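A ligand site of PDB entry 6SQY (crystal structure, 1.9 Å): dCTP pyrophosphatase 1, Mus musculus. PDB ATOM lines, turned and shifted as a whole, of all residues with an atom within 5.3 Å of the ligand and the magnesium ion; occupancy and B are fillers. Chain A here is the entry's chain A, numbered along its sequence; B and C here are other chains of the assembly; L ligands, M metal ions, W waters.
The side-chain carboxylate of Asp 98 is in hydrogen-bond range of an oxygen (O3) of the ligand.
The side-chain hydroxyl (OH) of Tyr 129 of chain B lies within hydrogen-bond range of an oxygen (O5) of the ligand, at 2.5 Å.
N2 of the ligand is in hydrogen-bond range of NE2 of His 51, 2.9 Å away.
ND2 of Asn 125 of chain B lies within hydrogen-bond range of O3 of the ligand.
O1 of the ligand sits at hydrogen-bond distance from NE2 of His 38, 2.7 Å away.
OD1 of Asn 125 of chain B is in hydrogen-bond range of NZ of Lys 121 of chain B, 2.9 Å away.
The side-chain amino group of Lys 121 of chain B is in salt-bridge range of the side-chain carboxylate of Asp 98 (2.8 Å).
The side-chain amide nitrogen (NE2) of Gln 72 of chain C lies close to the indole nitrogen (NE1) of Trp 73 of chain C, 3.2 Å away.
The side-chain hydroxyl (OH) of Tyr 102 sits close to a nitrogen (N1) of the ligand.
Merely in contact with the ligand: Phe 41, Trp 47, Ile 101, Lys 121 of chain B and Trp 73 of chain C.
Hydrophobic or aromatic side chains that line the ligand: His 38, Phe 41, Trp 47, His 51, Ile 101, Tyr 102, Tyr 129 of chain B and Trp 73 of chain C.
Of the 19 residues printed, 11 come within 4 Å of the ligand.
Four residues have an atom within 4 Å of the magnesium ion: Glu 63, Glu 66, Glu 95 and Asp 98.
OE1 of Glu 95 binds the magnesium ion (2.0 Å).
OE1 of Glu 63 is bound to the magnesium ion (2.1 Å).
The magnesium ion is bound by water W5 (2.1 Å).
The magnesium ion is bound by OE2 of Glu 66 (2.1 Å).
Water W2 binds the magnesium ion, at 2.2 Å.
OD2 of Asp 98 binds the magnesium ion (2.3 Å).
The magnesium ion has six donor atoms within binding distance.
Water W5 lies within hydrogen-bond range of OE2 of Glu 63 (2.8 Å) and O6 of the ligand (2.9 Å).
Water W3 lies within hydrogen-bond range of an oxygen (O7) of the ligand (2.7 Å), the side-chain carboxylate of Glu 63 (2.8 Å), the side-chain hydroxyl of Tyr 102 (2.8 Å) and the side-chain amide nitrogen of Gln 72 of chain C (3.1 Å).
Water W1 bridges an oxygen (O6) of the ligand and the side-chain amino group of Lys 121 of chain B.
Water W4 lies within hydrogen-bond range of an oxygen (O7) of the ligand and the indole nitrogen of Trp 73 of chain C.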
ATOM      1  N   HIS A  38      -6.285  23.409   9.918  1.00  0.00           N
ATOM      2  CA  HIS A  38      -5.570  23.405   8.669  1.00  0.00           C
ATOM      3  C   HIS A  38      -5.994  22.235   7.806  1.00  0.00           C
ATOM      4  O   HIS A  38      -6.171  22.386   6.591  1.00  0.00           O
ATOM      5  CB  HIS A  38      -4.040  23.362   8.857  1.00  0.00           C
ATOM      6  CG  HIS A  38      -3.315  23.440   7.570  1.00  0.00           C
ATOM      7  ND1 HIS A  38      -2.784  22.324   6.954  1.00  0.00           N
ATOM      8  CD2 HIS A  38      -3.139  24.470   6.722  1.00  0.00           C
ATOM      9  CE1 HIS A  38      -2.262  22.686   5.803  1.00  0.00           C
ATOM     10  NE2 HIS A  38      -2.460  23.994   5.637  1.00  0.00           N
ATOM     11  N   PHE A  41      -9.380  23.000   6.188  1.00  0.00           N
ATOM     12  CA  PHE A  41      -9.087  23.995   5.147  1.00  0.00           C
ATOM     13  C   PHE A  41      -8.521  23.363   3.881  1.00  0.00           C
ATOM     14  O   PHE A  41      -8.962  23.669   2.760  1.00  0.00           O
ATOM     15  CB  PHE A  41      -8.130  25.079   5.727  1.00  0.00           C
ATOM     16  CG  PHE A  41      -7.564  26.052   4.708  1.00  0.00           C
ATOM     17  CD1 PHE A  41      -8.271  27.181   4.331  1.00  0.00           C
ATOM     18  CD2 PHE A  41      -6.291  25.846   4.166  1.00  0.00           C
ATOM     19  CE1 PHE A  41      -7.745  28.084   3.405  1.00  0.00           C
ATOM     20  CE2 PHE A  41      -5.765  26.749   3.240  1.00  0.00           C
ATOM     21  CZ  PHE A  41      -6.489  27.860   2.860  1.00  0.00           C
ATOM     22  N   TRP A  47      -6.538  19.946  -1.482  1.00  0.00           N
ATOM     23  CA  TRP A  47      -5.118  20.328  -1.534  1.00  0.00           C
ATOM     24  C   TRP A  47      -4.140  19.316  -0.915  1.00  0.00           C
ATOM     25  O   TRP A  47      -2.916  19.553  -0.895  1.00  0.00           O
ATOM     26  CB  TRP A  47      -4.957  21.700  -0.871  1.00  0.00           C
ATOM     27  CG  TRP A  47      -5.330  22.859  -1.749  1.00  0.00           C
ATOM     28  CD1 TRP A  47      -5.740  22.837  -3.056  1.00  0.00           C
ATOM     29  CD2 TRP A  47      -5.289  24.240  -1.382  1.00  0.00           C
ATOM     30  NE1 TRP A  47      -5.966  24.103  -3.509  1.00  0.00           N
ATOM     31  CE2 TRP A  47      -5.701  24.986  -2.504  1.00  0.00           C
ATOM     32  CE3 TRP A  47      -4.931  24.914  -0.224  1.00  0.00           C
ATOM     33  CZ2 TRP A  47      -5.768  26.370  -2.485  1.00  0.00           C
ATOM     34  CZ3 TRP A  47      -5.015  26.281  -0.207  1.00  0.00           C
ATOM     35  CH2 TRP A  47      -5.426  26.997  -1.327  1.00  0.00           C
ATOM     36  N   PHE A  50      -0.989  18.564  -2.772  1.00  0.00           N
ATOM     37  CA  PHE A  50       0.083  19.547  -2.725  1.00  0.00           C
ATOM     38  C   PHE A  50       0.846  19.464  -1.389  1.00  0.00           C
ATOM     39  O   PHE A  50       1.939  19.976  -1.297  1.00  0.00           O
ATOM     40  CB  PHE A  50      -0.436  20.966  -2.861  1.00  0.00           C
ATOM     41  CG  PHE A  50      -1.054  21.283  -4.181  1.00  0.00           C
ATOM     42  CD1 PHE A  50      -0.243  21.612  -5.254  1.00  0.00           C
ATOM     43  CD2 PHE A  50      -2.447  21.316  -4.351  1.00  0.00           C
ATOM     44  CE1 PHE A  50      -0.799  21.951  -6.501  1.00  0.00           C
ATOM     45  CE2 PHE A  50      -3.005  21.607  -5.572  1.00  0.00           C
ATOM     46  CZ  PHE A  50      -2.189  21.949  -6.647  1.00  0.00           C
ATOM     47  N   HIS A  51       0.278  18.859  -0.352  1.00  0.00           N
ATOM     48  CA  HIS A  51       0.845  18.926   0.979  1.00  0.00           C
ATOM     49  C   HIS A  51       1.726  17.719   1.337  1.00  0.00           C
ATOM     50  O   HIS A  51       1.651  17.182   2.448  1.00  0.00           O
ATOM     51  CB  HIS A  51      -0.286  19.142   1.985  1.00  0.00           C
ATOM     52  CG  HIS A  51      -0.915  20.491   1.898  1.00  0.00           C
ATOM     53  ND1 HIS A  51      -2.029  20.832   2.622  1.00  0.00           N
ATOM     54  CD2 HIS A  51      -0.576  21.596   1.185  1.00  0.00           C
ATOM     55  CE1 HIS A  51      -2.352  22.097   2.361  1.00  0.00           C
ATOM     56  NE2 HIS A  51      -1.476  22.580   1.500  1.00  0.00           N
ATOM     57  N   GLU A  63       8.038  31.073   4.141  1.00  0.00           N
ATOM     58  CA  GLU A  63       7.407  31.909   5.177  1.00  0.00           C
ATOM     59  C   GLU A  63       8.456  32.439   6.151  1.00  0.00           C
ATOM     60  O   GLU A  63       8.367  33.551   6.603  1.00  0.00           O
ATOM     61  CB  GLU A  63       6.303  31.150   5.918  1.00  0.00           C
ATOM     62  CG  GLU A  63       5.162  30.630   5.019  1.00  0.00           C
ATOM     63  CD  GLU A  63       4.457  31.692   4.199  1.00  0.00           C
ATOM     64  OE1 GLU A  63       4.553  32.912   4.512  1.00  0.00           O
ATOM     65  OE2 GLU A  63       3.776  31.303   3.229  1.00  0.00           O
ATOM     66  N   GLU A  66       9.798  35.462   4.439  1.00  0.00           N
ATOM     67  CA  GLU A  66       8.921  36.613   4.619  1.00  0.00           C
ATOM     68  C   GLU A  66       9.024  37.231   6.026  1.00  0.00           C
ATOM     69  O   GLU A  66       9.002  38.435   6.175  1.00  0.00           O
ATOM     70  CB  GLU A  66       7.454  36.272   4.294  1.00  0.00           C
ATOM     71  CG  GLU A  66       7.280  35.998   2.791  1.00  0.00           C
ATOM     72  CD  GLU A  66       5.783  35.947   2.344  1.00  0.00           C
ATOM     73  OE1 GLU A  66       5.472  36.485   1.286  1.00  0.00           O
ATOM     74  OE2 GLU A  66       4.910  35.468   3.081  1.00  0.00           O
ATOM     75  N   GLU A  94       0.902  38.024  10.903  1.00  0.00           N
ATOM     76  CA  GLU A  94       0.620  37.181   9.774  1.00  0.00           C
ATOM     77  C   GLU A  94       1.751  36.227   9.441  1.00  0.00           C
ATOM     78  O   GLU A  94       1.493  35.031   9.258  1.00  0.00           O
ATOM     79  CB  GLU A  94       0.242  37.983   8.546  1.00  0.00           C
ATOM     80  CG  GLU A  94      -1.133  38.662   8.734  1.00  0.00           C
ATOM     81  CD  GLU A  94      -1.439  39.623   7.622  1.00  0.00           C
ATOM     82  OE1 GLU A  94      -2.017  40.696   7.897  1.00  0.00           O
ATOM     83  OE2 GLU A  94      -1.071  39.331   6.473  1.00  0.00           O
ATOM     84  N   GLU A  95       2.989  36.727   9.399  1.00  0.00           N
ATOM     85  CA  GLU A  95       4.099  35.862   9.018  1.00  0.00           C
ATOM     86  C   GLU A  95       4.477  34.868  10.112  1.00  0.00           C
ATOM     87  O   GLU A  95       4.736  33.693   9.791  1.00  0.00           O
ATOM     88  CB  GLU A  95       5.337  36.639   8.532  1.00  0.00           C
ATOM     89  CG  GLU A  95       5.114  37.565   7.350  1.00  0.00           C
ATOM     90  CD  GLU A  95       4.282  37.007   6.186  1.00  0.00           C
ATOM     91  OE1 GLU A  95       4.322  35.799   5.895  1.00  0.00           O
ATOM     92  OE2 GLU A  95       3.602  37.784   5.516  1.00  0.00           O
ATOM     93  N   SER A  97       2.304  33.569  12.030  1.00  0.00           N
ATOM     94  CA  SER A  97       1.230  32.595  11.889  1.00  0.00           C
ATOM     95  C   SER A  97       1.474  31.662  10.704  1.00  0.00           C
ATOM     96  O   SER A  97       1.252  30.457  10.833  1.00  0.00           O
ATOM     97  CB  SER A  97      -0.144  33.288  11.721  1.00  0.00           C
ATOM     98  OG  SER A  97      -0.467  34.061  12.877  1.00  0.00           O
ATOM     99  N   ASP A  98       1.894  32.198   9.550  1.00  0.00           N
ATOM    100  CA  ASP A  98       2.162  31.359   8.389  1.00  0.00           C
ATOM    101  C   ASP A  98       3.260  30.316   8.691  1.00  0.00           C
ATOM    102  O   ASP A  98       3.136  29.161   8.262  1.00  0.00           O
ATOM    103  CB  ASP A  98       2.599  32.146   7.151  1.00  0.00           C
ATOM    104  CG  ASP A  98       1.500  32.892   6.456  1.00  0.00           C
ATOM    105  OD1 ASP A  98       0.329  32.514   6.598  1.00  0.00           O
ATOM    106  OD2 ASP A  98       1.840  33.870   5.747  1.00  0.00           O
ATOM    107  N   ILE A 101       1.611  27.600  10.976  1.00  0.00           N
ATOM    108  CA  ILE A 101       0.647  26.770  10.223  1.00  0.00           C
ATOM    109  C   ILE A 101       1.378  25.675   9.415  1.00  0.00           C
ATOM    110  O   ILE A 101       1.062  24.482   9.532  1.00  0.00           O
ATOM    111  CB  ILE A 101      -0.285  27.631   9.341  1.00  0.00           C
ATOM    112  CG1 ILE A 101      -1.224  28.449  10.221  1.00  0.00           C
ATOM    113  CG2 ILE A 101      -1.042  26.793   8.361  1.00  0.00           C
ATOM    114  CD1 ILE A 101      -1.777  29.648   9.533  1.00  0.00           C
ATOM    115  N   TYR A 102       2.407  26.058   8.657  1.00  0.00           N
ATOM    116  CA  TYR A 102       3.169  25.049   7.930  1.00  0.00           C
ATOM    117  C   TYR A 102       3.955  24.099   8.818  1.00  0.00           C
ATOM    118  O   TYR A 102       4.099  22.942   8.475  1.00  0.00           O
ATOM    119  CB  TYR A 102       4.070  25.660   6.828  1.00  0.00           C
ATOM    120  CG  TYR A 102       3.317  26.186   5.631  1.00  0.00           C
ATOM    121  CD1 TYR A 102       2.503  25.361   4.871  1.00  0.00           C
ATOM    122  CD2 TYR A 102       3.413  27.520   5.248  1.00  0.00           C
ATOM    123  CE1 TYR A 102       1.823  25.847   3.750  1.00  0.00           C
ATOM    124  CE2 TYR A 102       2.750  27.981   4.148  1.00  0.00           C
ATOM    125  CZ  TYR A 102       1.957  27.151   3.399  1.00  0.00           C
ATOM    126  OH  TYR A 102       1.327  27.658   2.274  1.00  0.00           O
ATOM    127  N   LYS B 121      -5.229  34.691  10.746  1.00  0.00           N
ATOM    128  CA  LYS B 121      -4.596  34.297   9.468  1.00  0.00           C
ATOM    129  C   LYS B 121      -5.410  33.248   8.712  1.00  0.00           C
ATOM    130  O   LYS B 121      -5.562  33.346   7.497  1.00  0.00           O
ATOM    131  CB  LYS B 121      -3.134  33.832   9.642  1.00  0.00           C
ATOM    132  CG  LYS B 121      -2.334  33.793   8.336  1.00  0.00           C
ATOM    133  CD  LYS B 121      -2.361  35.126   7.586  1.00  0.00           C
ATOM    134  CE  LYS B 121      -1.436  35.214   6.390  1.00  0.00           C
ATOM    135  NZ  LYS B 121      -1.601  34.121   5.385  1.00  0.00           N
ATOM    136  N   ASN B 125      -6.854  33.468   5.117  1.00  0.00           N
ATOM    137  CA  ASN B 125      -6.585  32.416   4.133  1.00  0.00           C
ATOM    138  C   ASN B 125      -7.903  31.978   3.419  1.00  0.00           C
ATOM    139  O   ASN B 125      -7.940  31.827   2.175  1.00  0.00           O
ATOM    140  CB  ASN B 125      -5.921  31.210   4.801  1.00  0.00           C
ATOM    141  CG  ASN B 125      -4.491  31.481   5.233  1.00  0.00           C
ATOM    142  OD1 ASN B 125      -3.909  32.490   4.837  1.00  0.00           O
ATOM    143  ND2 ASN B 125      -3.931  30.605   6.093  1.00  0.00           N
ATOM    144  N   ARG B 128      -8.868  34.713   0.888  1.00  0.00           N
ATOM    145  CA  ARG B 128      -8.013  34.719  -0.302  1.00  0.00           C
ATOM    146  C   ARG B 128      -8.239  33.525  -1.215  1.00  0.00           C
ATOM    147  O   ARG B 128      -8.061  33.644  -2.408  1.00  0.00           O
ATOM    148  CB  ARG B 128      -6.523  34.796   0.049  1.00  0.00           C
ATOM    149  CG  ARG B 128      -6.106  36.068   0.723  1.00  0.00           C
ATOM    150  CD  ARG B 128      -4.574  36.176   0.876  1.00  0.00           C
ATOM    151  NE  ARG B 128      -4.167  37.057   1.970  1.00  0.00           N
ATOM    152  CZ  ARG B 128      -4.260  38.398   1.991  1.00  0.00           C
ATOM    153  NH1 ARG B 128      -4.765  39.080   0.949  1.00  0.00           N
ATOM    154  NH2 ARG B 128      -3.842  39.058   3.080  1.00  0.00           N
ATOM    155  N   TYR B 129      -8.646  32.394  -0.667  1.00  0.00           N
ATOM    156  CA  TYR B 129      -8.885  31.174  -1.474  1.00  0.00           C
ATOM    157  C   TYR B 129     -10.286  30.580  -1.254  1.00  0.00           C
ATOM    158  O   TYR B 129     -10.437  29.513  -0.646  1.00  0.00           O
ATOM    159  CB  TYR B 129      -7.852  30.125  -1.093  1.00  0.00           C
ATOM    160  CG  TYR B 129      -6.434  30.474  -1.424  1.00  0.00           C
ATOM    161  CD1 TYR B 129      -5.944  30.336  -2.734  1.00  0.00           C
ATOM    162  CD2 TYR B 129      -5.548  30.881  -0.408  1.00  0.00           C
ATOM    163  CE1 TYR B 129      -4.618  30.620  -3.034  1.00  0.00           C
ATOM    164  CE2 TYR B 129      -4.200  31.160  -0.698  1.00  0.00           C
ATOM    165  CZ  TYR B 129      -3.751  31.028  -2.008  1.00  0.00           C
ATOM    166  OH  TYR B 129      -2.435  31.271  -2.353  1.00  0.00           O
ATOM    167  N   GLN C  72       8.048  25.387  -4.263  1.00  0.00           N
ATOM    168  CA  GLN C  72       7.311  24.786  -3.151  1.00  0.00           C
ATOM    169  C   GLN C  72       6.150  23.898  -3.550  1.00  0.00           C
ATOM    170  O   GLN C  72       5.922  22.899  -2.897  1.00  0.00           O
ATOM    171  CB  GLN C  72       6.860  25.842  -2.118  1.00  0.00           C
ATOM    172  CG  GLN C  72       5.801  26.864  -2.535  1.00  0.00           C
ATOM    173  CD  GLN C  72       5.569  27.912  -1.450  1.00  0.00           C
ATOM    174  OE1 GLN C  72       6.499  28.500  -0.935  1.00  0.00           O
ATOM    175  NE2 GLN C  72       4.323  28.099  -1.033  1.00  0.00           N
ATOM    176  N   TRP C  73       5.439  24.229  -4.615  1.00  0.00           N
ATOM    177  CA  TRP C  73       4.244  23.464  -5.012  1.00  0.00           C
ATOM    178  C   TRP C  73       4.486  22.572  -6.229  1.00  0.00           C
ATOM    179  O   TRP C  73       3.532  22.001  -6.732  1.00  0.00           O
ATOM    180  CB  TRP C  73       3.057  24.377  -5.272  1.00  0.00           C
ATOM    181  CG  TRP C  73       2.634  25.209  -4.131  1.00  0.00           C
ATOM    182  CD1 TRP C  73       2.379  26.509  -4.169  1.00  0.00           C
ATOM    183  CD2 TRP C  73       2.410  24.789  -2.793  1.00  0.00           C
ATOM    184  NE1 TRP C  73       1.980  26.957  -2.941  1.00  0.00           N
ATOM    185  CE2 TRP C  73       2.028  25.913  -2.069  1.00  0.00           C
ATOM    186  CE3 TRP C  73       2.538  23.571  -2.123  1.00  0.00           C
ATOM    187  CZ2 TRP C  73       1.725  25.880  -0.707  1.00  0.00           C
ATOM    188  CZ3 TRP C  73       2.240  23.528  -0.769  1.00  0.00           C
ATOM    189  CH2 TRP C  73       1.851  24.679  -0.075  1.00  0.00           C
HETATM  190  N1  LIG L   1      -2.090  27.663   2.370  1.00  0.00           N
HETATM  191  C1  LIG L   1      -1.964  26.240   2.466  1.00  0.00           C
HETATM  192  N2  LIG L   1      -1.745  25.489   1.342  1.00  0.00           N
HETATM  193  C2  LIG L   1      -1.670  26.083   0.111  1.00  0.00           C
HETATM  194  C3  LIG L   1      -1.810  27.477  -0.008  1.00  0.00           C
HETATM  195  C4  LIG L   1      -2.019  28.250   1.133  1.00  0.00           C
HETATM  196  O1  LIG L   1      -2.006  25.690   3.607  1.00  0.00           O
HETATM  197  N3  LIG L   1      -1.454  25.356  -1.007  1.00  0.00           N
HETATM  198  C5  LIG L   1      -2.311  28.495   3.580  1.00  0.00           C
HETATM  199  C6  LIG L   1      -1.234  28.377   4.679  1.00  0.00           C
HETATM  200  C7  LIG L   1      -0.650  29.786   4.918  1.00  0.00           C
HETATM  201  C8  LIG L   1      -1.210  30.637   3.786  1.00  0.00           C
HETATM  202  O2  LIG L   1      -2.328  29.896   3.213  1.00  0.00           O
HETATM  203  O3  LIG L   1      -1.024  30.389   6.179  1.00  0.00           O
HETATM  204  C9  LIG L   1      -0.182  30.974   2.714  1.00  0.00           C
HETATM  205  O4  LIG L   1      -0.873  31.596   1.634  1.00  0.00           O
HETATM  206  P1  LIG L   1      -0.094  32.347   0.414  1.00  0.00           P
HETATM  207  O5  LIG L   1      -1.216  32.501  -0.586  1.00  0.00           O
HETATM  208  O6  LIG L   1       0.318  33.658   1.042  1.00  0.00           O
HETATM  209  O7  LIG L   1       1.065  31.375   0.019  1.00  0.00           O
HETATM  210 MG    MG M   1       3.494  34.671   4.420  1.00  0.00          MG
HETATM  211  O   HOH W   1      -0.374  35.236   3.071  1.00  0.00           O
HETATM  212  O   HOH W   2       2.238  36.342   3.687  1.00  0.00           O
HETATM  213  O   HOH W   3       2.828  29.730   1.137  1.00  0.00           O
HETATM  214  O   HOH W   4       0.971  30.011  -2.363  1.00  0.00           O
HETATM  215  O   HOH W   5       2.644  33.796   2.746  1.00  0.00           O
HETATM  216  O   HOH W   6       3.406  32.604  -0.711  1.00  0.00           O
HETATM  217  O   HOH W   7       1.553  35.621  -0.129  1.00  0.00           O
